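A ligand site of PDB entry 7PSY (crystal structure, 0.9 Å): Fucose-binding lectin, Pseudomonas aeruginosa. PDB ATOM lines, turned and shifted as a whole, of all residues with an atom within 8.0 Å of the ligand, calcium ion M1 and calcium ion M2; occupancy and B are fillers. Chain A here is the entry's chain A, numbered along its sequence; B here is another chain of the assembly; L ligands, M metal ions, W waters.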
ATOM      1  N   ALA A  21      31.851  11.572  24.150  1.00  0.00           N
ATOM      2  CA  ALA A  21      30.411  11.571  24.379  1.00  0.00           C
ATOM      3  C   ALA A  21      30.052  12.120  25.753  1.00  0.00           C
ATOM      4  O   ALA A  21      30.725  11.839  26.759  1.00  0.00           O
ATOM      5  CB  ALA A  21      29.819  10.183  24.209  1.00  0.00           C
ATOM      6  N   ASN A  22      28.936  12.901  25.785  1.00  0.00           N
ATOM      7  CA  ASN A  22      28.411  13.491  27.007  1.00  0.00           C
ATOM      8  C   ASN A  22      26.884  13.557  26.904  1.00  0.00           C
ATOM      9  O   ASN A  22      26.319  14.639  26.730  1.00  0.00           O
ATOM     10  CB  ASN A  22      28.951  14.890  27.268  1.00  0.00           C
ATOM     11  CG  ASN A  22      30.418  14.897  27.596  1.00  0.00           C
ATOM     12  OD1 ASN A  22      30.822  14.609  28.709  1.00  0.00           O
ATOM     13  ND2 ASN A  22      31.236  15.238  26.588  1.00  0.00           N
ATOM     14  N   SER A  23      26.203  12.415  27.004  1.00  0.00           N
ATOM     15  CA  SER A  23      24.754  12.376  26.816  1.00  0.00           C
ATOM     16  C   SER A  23      24.200  11.035  27.256  1.00  0.00           C
ATOM     17  O   SER A  23      24.904  10.019  27.237  1.00  0.00           O
ATOM     18  CB  SER A  23      24.442  12.543  25.324  1.00  0.00           C
ATOM     19  OG  SER A  23      23.055  12.373  25.106  1.00  0.00           O
ATOM     20  N   SER A  24      22.919  11.027  27.614  1.00  0.00           N
ATOM     21  CA  SER A  24      22.194   9.771  27.806  1.00  0.00           C
ATOM     22  C   SER A  24      22.242   8.892  26.559  1.00  0.00           C
ATOM     23  O   SER A  24      22.270   7.663  26.663  1.00  0.00           O
ATOM     24  CB  SER A  24      20.734  10.074  28.172  1.00  0.00           C
ATOM     25  OG  SER A  24      20.014  10.728  27.123  1.00  0.00           O
ATOM     26  N   GLY A  25      22.220   9.515  25.395  1.00  0.00           N
ATOM     27  CA  GLY A  25      22.021   8.800  24.151  1.00  0.00           C
ATOM     28  C   GLY A  25      23.312   8.321  23.526  1.00  0.00           C
ATOM     29  O   GLY A  25      24.338   8.993  23.589  1.00  0.00           O
ATOM     30  N   GLN A  27      25.878   8.088  20.758  1.00  0.00           N
ATOM     31  CA  GLN A  27      26.298   8.954  19.673  1.00  0.00           C
ATOM     32  C   GLN A  27      26.891   8.127  18.538  1.00  0.00           C
ATOM     33  O   GLN A  27      27.746   7.275  18.789  1.00  0.00           O
ATOM     34  CB  GLN A  27      27.368   9.923  20.177  1.00  0.00           C
ATOM     35  CG  GLN A  27      27.017  10.644  21.461  1.00  0.00           C
ATOM     36  CD  GLN A  27      25.902  11.662  21.274  1.00  0.00           C
ATOM     37  OE1 GLN A  27      26.013  12.545  20.428  1.00  0.00           O
ATOM     38  NE2 GLN A  27      24.857  11.548  22.082  1.00  0.00           N
ATOM     39  N   GLN A  44      28.439   5.506  24.124  1.00  0.00           N
ATOM     40  CA  GLN A  44      27.606   6.242  25.065  1.00  0.00           C
ATOM     41  C   GLN A  44      28.412   6.524  26.312  1.00  0.00           C
ATOM     42  O   GLN A  44      29.053   5.623  26.880  1.00  0.00           O
ATOM     43  CB  GLN A  44      26.325   5.459  25.396  1.00  0.00           C
ATOM     44  CG  GLN A  44      25.318   6.227  26.250  1.00  0.00           C
ATOM     45  CD  GLN A  44      25.658   6.247  27.718  1.00  0.00           C
ATOM     46  OE1 GLN A  44      26.071   5.226  28.268  1.00  0.00           O
ATOM     47  NE2 GLN A  44      25.429   7.374  28.374  1.00  0.00           N
ATOM     48  N   SER A  45      28.355   7.772  26.763  1.00  0.00           N
ATOM     49  CA  SER A  45      28.990   8.192  27.994  1.00  0.00           C
ATOM     50  C   SER A  45      28.342   9.490  28.439  1.00  0.00           C
ATOM     51  O   SER A  45      28.019  10.326  27.599  1.00  0.00           O
ATOM     52  CB  SER A  45      30.489   8.445  27.754  1.00  0.00           C
ATOM     53  OG  SER A  45      31.168   8.844  28.930  1.00  0.00           O
ATOM     54  N   THR A  46      28.281   9.706  29.756  1.00  0.00           N
ATOM     55  CA  THR A  46      28.023  11.025  30.325  1.00  0.00           C
ATOM     56  C   THR A  46      29.269  11.592  30.998  1.00  0.00           C
ATOM     57  O   THR A  46      29.202  12.573  31.734  1.00  0.00           O
ATOM     58  CB  THR A  46      26.851  10.997  31.315  1.00  0.00           C
ATOM     59  OG1 THR A  46      27.034   9.935  32.237  1.00  0.00           O
ATOM     60  CG2 THR A  46      25.536  10.801  30.588  1.00  0.00           C
ATOM     61  N   VAL A  70      21.914  10.685  16.735  1.00  0.00           N
ATOM     62  CA  VAL A  70      21.561  10.165  18.048  1.00  0.00           C
ATOM     63  C   VAL A  70      20.092   9.791  18.034  1.00  0.00           C
ATOM     64  O   VAL A  70      19.236  10.613  17.695  1.00  0.00           O
ATOM     65  CB  VAL A  70      21.794  11.206  19.161  1.00  0.00           C
ATOM     66  CG1 VAL A  70      21.440  10.632  20.535  1.00  0.00           C
ATOM     67  CG2 VAL A  70      23.209  11.699  19.125  1.00  0.00           C
ATOM     68  N   ASN A  71      19.795   8.574  18.478  1.00  0.00           N
ATOM     69  CA  ASN A  71      18.427   8.121  18.710  1.00  0.00           C
ATOM     70  C   ASN A  71      17.549   8.373  17.486  1.00  0.00           C
ATOM     71  O   ASN A  71      16.341   8.587  17.585  1.00  0.00           O
ATOM     72  CB  ASN A  71      17.866   8.699  20.011  1.00  0.00           C
ATOM     73  CG  ASN A  71      18.480   8.009  21.243  1.00  0.00           C
ATOM     74  OD1 ASN A  71      18.848   6.799  21.212  1.00  0.00           O
ATOM     75  ND2 ASN A  71      18.640   8.768  22.340  1.00  0.00           N
ATOM     76  N   SER A  95      27.928  19.232  19.276  1.00  0.00           N
ATOM     77  CA  SER A  95      26.670  18.780  18.729  1.00  0.00           C
ATOM     78  C   SER A  95      25.639  18.649  19.833  1.00  0.00           C
ATOM     79  O   SER A  95      25.979  18.353  20.981  1.00  0.00           O
ATOM     80  CB  SER A  95      26.847  17.451  17.986  1.00  0.00           C
ATOM     81  OG  SER A  95      27.220  16.376  18.849  1.00  0.00           O
ATOM     82  N   GLU A  96      24.377  18.899  19.460  1.00  0.00           N
ATOM     83  CA  GLU A  96      23.259  18.882  20.405  1.00  0.00           C
ATOM     84  C   GLU A  96      22.215  17.890  19.929  1.00  0.00           C
ATOM     85  O   GLU A  96      21.679  18.022  18.817  1.00  0.00           O
ATOM     86  CB  GLU A  96      22.656  20.278  20.524  1.00  0.00           C
ATOM     87  CG  GLU A  96      21.450  20.315  21.459  1.00  0.00           C
ATOM     88  CD  GLU A  96      21.755  19.773  22.834  1.00  0.00           C
ATOM     89  OE1 GLU A  96      22.800  20.157  23.435  1.00  0.00           O
ATOM     90  OE2 GLU A  96      21.029  18.895  23.327  1.00  0.00           O
ATOM     91  N   ASP A  97      21.920  16.911  20.774  1.00  0.00           N
ATOM     92  CA  ASP A  97      20.980  15.843  20.474  1.00  0.00           C
ATOM     93  C   ASP A  97      19.612  16.032  21.093  1.00  0.00           C
ATOM     94  O   ASP A  97      18.726  15.216  20.837  1.00  0.00           O
ATOM     95  CB  ASP A  97      21.596  14.485  20.866  1.00  0.00           C
ATOM     96  CG  ASP A  97      21.735  14.255  22.367  1.00  0.00           C
ATOM     97  OD1 ASP A  97      20.971  14.840  23.156  1.00  0.00           O
ATOM     98  OD2 ASP A  97      22.630  13.453  22.716  1.00  0.00           O
ATOM     99  N   GLY A  98      19.430  17.105  21.847  1.00  0.00           N
ATOM    100  CA  GLY A  98      18.258  17.282  22.677  1.00  0.00           C
ATOM    101  C   GLY A  98      17.849  18.723  22.783  1.00  0.00           C
ATOM    102  O   GLY A  98      17.835  19.450  21.783  1.00  0.00           O
ATOM    103  N   THR A  99      17.534  19.148  24.006  1.00  0.00           N
ATOM    104  CA  THR A  99      16.904  20.428  24.251  1.00  0.00           C
ATOM    105  C   THR A  99      17.718  21.350  25.159  1.00  0.00           C
ATOM    106  O   THR A  99      17.399  22.537  25.228  1.00  0.00           O
ATOM    107  CB  THR A  99      15.515  20.215  24.857  1.00  0.00           C
ATOM    108  OG1 THR A  99      15.667  19.494  26.077  1.00  0.00           O
ATOM    109  CG2 THR A  99      14.642  19.411  23.922  1.00  0.00           C
ATOM    110  N   ASP A 100      18.746  20.856  25.852  1.00  0.00           N
ATOM    111  CA  ASP A 100      19.429  21.691  26.831  1.00  0.00           C
ATOM    112  C   ASP A 100      20.498  22.605  26.235  1.00  0.00           C
ATOM    113  O   ASP A 100      20.994  23.482  26.936  1.00  0.00           O
ATOM    114  CB  ASP A 100      20.023  20.858  27.976  1.00  0.00           C
ATOM    115  CG  ASP A 100      21.187  19.950  27.563  1.00  0.00           C
ATOM    116  OD1 ASP A 100      21.406  19.753  26.355  1.00  0.00           O
ATOM    117  OD2 ASP A 100      21.855  19.422  28.475  1.00  0.00           O
ATOM    118  N   ASN A 101      20.859  22.403  24.974  1.00  0.00           N
ATOM    119  CA  ASN A 101      21.822  23.260  24.268  1.00  0.00           C
ATOM    120  C   ASN A 101      23.168  23.365  24.975  1.00  0.00           C
ATOM    121  O   ASN A 101      23.826  24.394  24.929  1.00  0.00           O
ATOM    122  CB  ASN A 101      21.199  24.632  23.985  1.00  0.00           C
ATOM    123  CG  ASN A 101      20.033  24.517  23.062  1.00  0.00           C
ATOM    124  OD1 ASN A 101      19.937  23.565  22.296  1.00  0.00           O
ATOM    125  ND2 ASN A 101      19.127  25.474  23.147  1.00  0.00           N
ATOM    126  N   ASP A 102      23.623  22.252  25.545  1.00  0.00           N
ATOM    127  CA  ASP A 102      25.010  22.205  25.997  1.00  0.00           C
ATOM    128  C   ASP A 102      25.992  21.945  24.850  1.00  0.00           C
ATOM    129  O   ASP A 102      27.174  22.277  24.984  1.00  0.00           O
ATOM    130  CB  ASP A 102      25.238  21.293  27.224  1.00  0.00           C
ATOM    131  CG  ASP A 102      24.985  19.791  26.983  1.00  0.00           C
ATOM    132  OD1 ASP A 102      24.514  19.414  25.882  1.00  0.00           O
ATOM    133  OD2 ASP A 102      25.240  19.036  27.950  1.00  0.00           O
ATOM    134  N   TYR A 103      25.532  21.370  23.743  1.00  0.00           N
ATOM    135  CA  TYR A 103      26.352  21.177  22.549  1.00  0.00           C
ATOM    136  C   TYR A 103      27.582  20.309  22.807  1.00  0.00           C
ATOM    137  O   TYR A 103      28.521  20.345  22.022  1.00  0.00           O
ATOM    138  CB  TYR A 103      26.695  22.503  21.853  1.00  0.00           C
ATOM    139  CG  TYR A 103      25.528  22.940  20.983  1.00  0.00           C
ATOM    140  CD1 TYR A 103      25.435  22.528  19.673  1.00  0.00           C
ATOM    141  CD2 TYR A 103      24.469  23.678  21.519  1.00  0.00           C
ATOM    142  CE1 TYR A 103      24.332  22.862  18.878  1.00  0.00           C
ATOM    143  CE2 TYR A 103      23.362  24.004  20.735  1.00  0.00           C
ATOM    144  CZ  TYR A 103      23.292  23.571  19.437  1.00  0.00           C
ATOM    145  OH  TYR A 103      22.178  23.883  18.704  1.00  0.00           O
ATOM    146  N   ASN A 104      27.547  19.470  23.835  1.00  0.00           N
ATOM    147  CA  ASN A 104      28.685  18.613  24.141  1.00  0.00           C
ATOM    148  C   ASN A 104      28.367  17.131  23.946  1.00  0.00           C
ATOM    149  O   ASN A 104      29.152  16.263  24.344  1.00  0.00           O
ATOM    150  CB  ASN A 104      29.197  18.840  25.560  1.00  0.00           C
ATOM    151  CG  ASN A 104      28.244  18.274  26.597  1.00  0.00           C
ATOM    152  OD1 ASN A 104      27.197  17.745  26.237  1.00  0.00           O
ATOM    153  ND2 ASN A 104      28.622  18.331  27.867  1.00  0.00           N
ATOM    154  N   ASP A 105      27.230  16.833  23.330  1.00  0.00           N
ATOM    155  CA  ASP A 105      26.703  15.485  23.389  1.00  0.00           C
ATOM    156  C   ASP A 105      27.604  14.510  22.653  1.00  0.00           C
ATOM    157  O   ASP A 105      27.885  13.407  23.139  1.00  0.00           O
ATOM    158  CB  ASP A 105      25.272  15.477  22.879  1.00  0.00           C
ATOM    159  CG  ASP A 105      24.356  16.345  23.722  1.00  0.00           C
ATOM    160  OD1 ASP A 105      24.525  16.411  24.958  1.00  0.00           O
ATOM    161  OD2 ASP A 105      23.420  16.999  23.146  1.00  0.00           O
ATOM    162  N   ALA A 106      28.080  14.939  21.493  1.00  0.00           N
ATOM    163  CA  ALA A 106      29.295  14.423  20.876  1.00  0.00           C
ATOM    164  C   ALA A 106      30.179  15.626  20.592  1.00  0.00           C
ATOM    165  O   ALA A 106      29.718  16.606  19.994  1.00  0.00           O
ATOM    166  CB  ALA A 106      29.071  13.629  19.610  1.00  0.00           C
ATOM    167  N   PRO B 113      31.565  22.369  29.260  1.00  0.00           N
ATOM    168  CA  PRO B 113      31.215  21.432  30.336  1.00  0.00           C
ATOM    169  C   PRO B 113      31.077  20.007  29.819  1.00  0.00           C
ATOM    170  O   PRO B 113      30.996  19.766  28.613  1.00  0.00           O
ATOM    171  CB  PRO B 113      29.867  21.965  30.824  1.00  0.00           C
ATOM    172  CG  PRO B 113      29.264  22.515  29.584  1.00  0.00           C
ATOM    173  CD  PRO B 113      30.386  23.129  28.783  1.00  0.00           C
ATOM    174  N   LEU B 114      31.005  19.093  30.766  1.00  0.00           N
ATOM    175  CA  LEU B 114      30.772  17.682  30.527  1.00  0.00           C
ATOM    176  C   LEU B 114      29.343  17.316  30.894  1.00  0.00           C
ATOM    177  O   LEU B 114      28.551  18.142  31.373  1.00  0.00           O
ATOM    178  CB  LEU B 114      31.756  16.824  31.329  1.00  0.00           C
ATOM    179  CG  LEU B 114      33.232  17.165  31.118  1.00  0.00           C
ATOM    180  CD1 LEU B 114      34.068  16.105  31.860  1.00  0.00           C
ATOM    181  CD2 LEU B 114      33.611  17.220  29.669  1.00  0.00           C
ATOM    182  N   GLY B 115      28.988  16.070  30.632  1.00  0.00           N
ATOM    183  CA  GLY B 115      27.713  15.518  31.072  1.00  0.00           C
ATOM    184  C   GLY B 115      26.572  15.659  30.101  1.00  0.00           C
ATOM    185  O   GLY B 115      26.587  16.485  29.186  1.00  0.00           O
ATOM    186  OXT GLY B 115      25.600  14.904  30.336  1.00  0.00           O
HETATM  187  C1  LIG L   1      20.881  14.273  26.872  1.00  0.00           C
HETATM  188  C2  LIG L   1      21.782  15.453  26.476  1.00  0.00           C
HETATM  189  C3  LIG L   1      21.978  16.357  27.675  1.00  0.00           C
HETATM  190  C4  LIG L   1      22.572  15.588  28.831  1.00  0.00           C
HETATM  191  C5  LIG L   1      21.685  14.377  29.126  1.00  0.00           C
HETATM  192  C6  LIG L   1      22.279  13.469  30.187  1.00  0.00           C
HETATM  193  O1  LIG L   1      19.622  14.809  27.220  1.00  0.00           O
HETATM  194  O2  LIG L   1      21.224  16.239  25.401  1.00  0.00           O
HETATM  195  O3  LIG L   1      22.893  17.394  27.289  1.00  0.00           O
HETATM  196  O4  LIG L   1      23.889  15.199  28.449  1.00  0.00           O
HETATM  197  O5  LIG L   1      21.473  13.582  27.947  1.00  0.00           O
HETATM  198 CA    CA M   1      22.639  18.286  25.007  1.00  0.00          CA
HETATM  199 CA    CA M   2      25.292  16.734  27.160  1.00  0.00          CA
HETATM  200  O   HOH W   1      18.774  17.712  26.147  1.00  0.00           O
HETATM  201  O   HOH W   2      18.137  12.469  27.277  1.00  0.00           O
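O2 of the ligand lies close to OD1 of Asp 97 (2.7 Å).
OG of Ser 23 sits close to O5 of the ligand (3.5 Å).
OG of Ser 24 lies within hydrogen-bond range of O5 of the ligand (3.3 Å).
The backbone NH of Ser 24 sits at hydrogen-bond distance from an oxygen (O5) of the ligand, 3.0 Å away.
The side-chain amide nitrogen of Asn 104 sits at hydrogen-bond distance from the backbone carbonyl oxygen of Pro 113 of chain B (2.9 Å).
O of Asp 105 sits close to OE1 of Gln 27 (3.4 Å).
The backbone NH (N) of Asn 101 lies close to the side-chain carboxylate (OE1) of Glu 96 (3.3 Å).
The side-chain carboxylate of Asp 97 lies within hydrogen-bond range of the side-chain hydroxyl of Ser 23, at 2.7 Å.
OE2 of Glu 96 sits close to N of Gly 98 (2.8 Å).
O of Ser 45 sits at hydrogen-bond distance from N of Ser 23, at 2.8 Å.
N of Asp 105 lies within hydrogen-bond range of O of Ser 95, at 3.1 Å.
The side-chain carboxylate (OD2) of Asp 97 sits at hydrogen-bond distance from the side-chain amide nitrogen (NE2) of Gln 27, 3.0 Å away.
Five residues have an atom within 4 Å of calcium ion M2: Asn 22, Asp 102, Asn 104, Asp 105 and Gly 115 of chain B.
The nearest printed residue that does not touch calcium ion M2 is Ser 23 (4.4 Å).
OD1 of Asp 100 binds calcium ion M1, at 2.3 Å.
OD1 of Asp 102 binds calcium ion M1 (2.4 Å).
Calcium ion M1 is bound by OD2 of Asp 105.
Calcium ion M1 is bound by the side-chain carboxylate (OE2) of Glu 96.
OE1 of Glu 96 binds calcium ion M1, at 2.4 Å.
O3 of the ligand binds calcium ion M1.
O2 of the ligand is bound to calcium ion M1, at 2.5 Å.
The side-chain carboxylate (OD1) of Asp 105 is bound to calcium ion M1 (2.7 Å).
Calcium ion M2 is bound by the side-chain amide oxygen of Asn 104 (2.3 Å), the side-chain carboxylate of Asp 105 (2.4 Å), the backbone carbonyl oxygen of Asn 22 (2.4 Å), the chain-end carboxylate of Gly 115 of chain B (2.4 Å), the side-chain carboxylate of Asp 102 (2.4 Å), an oxygen (O4) of the ligand (2.4 Å) and an oxygen (O3) of the ligand (2.5 Å).
Slightly farther from calcium ion M2 lies OD1 of Asp 102 (3.1 Å).
Water W2 lies within hydrogen-bond range of OG of Ser 24 (2.6 Å) and O1 of the ligand (2.8 Å).
Water W1 lies within hydrogen-bond range of the backbone NH of Thr 99 (2.9 Å), the backbone NH of Asp 100 (3.2 Å) and an oxygen (O1) of the ligand (3.2 Å).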
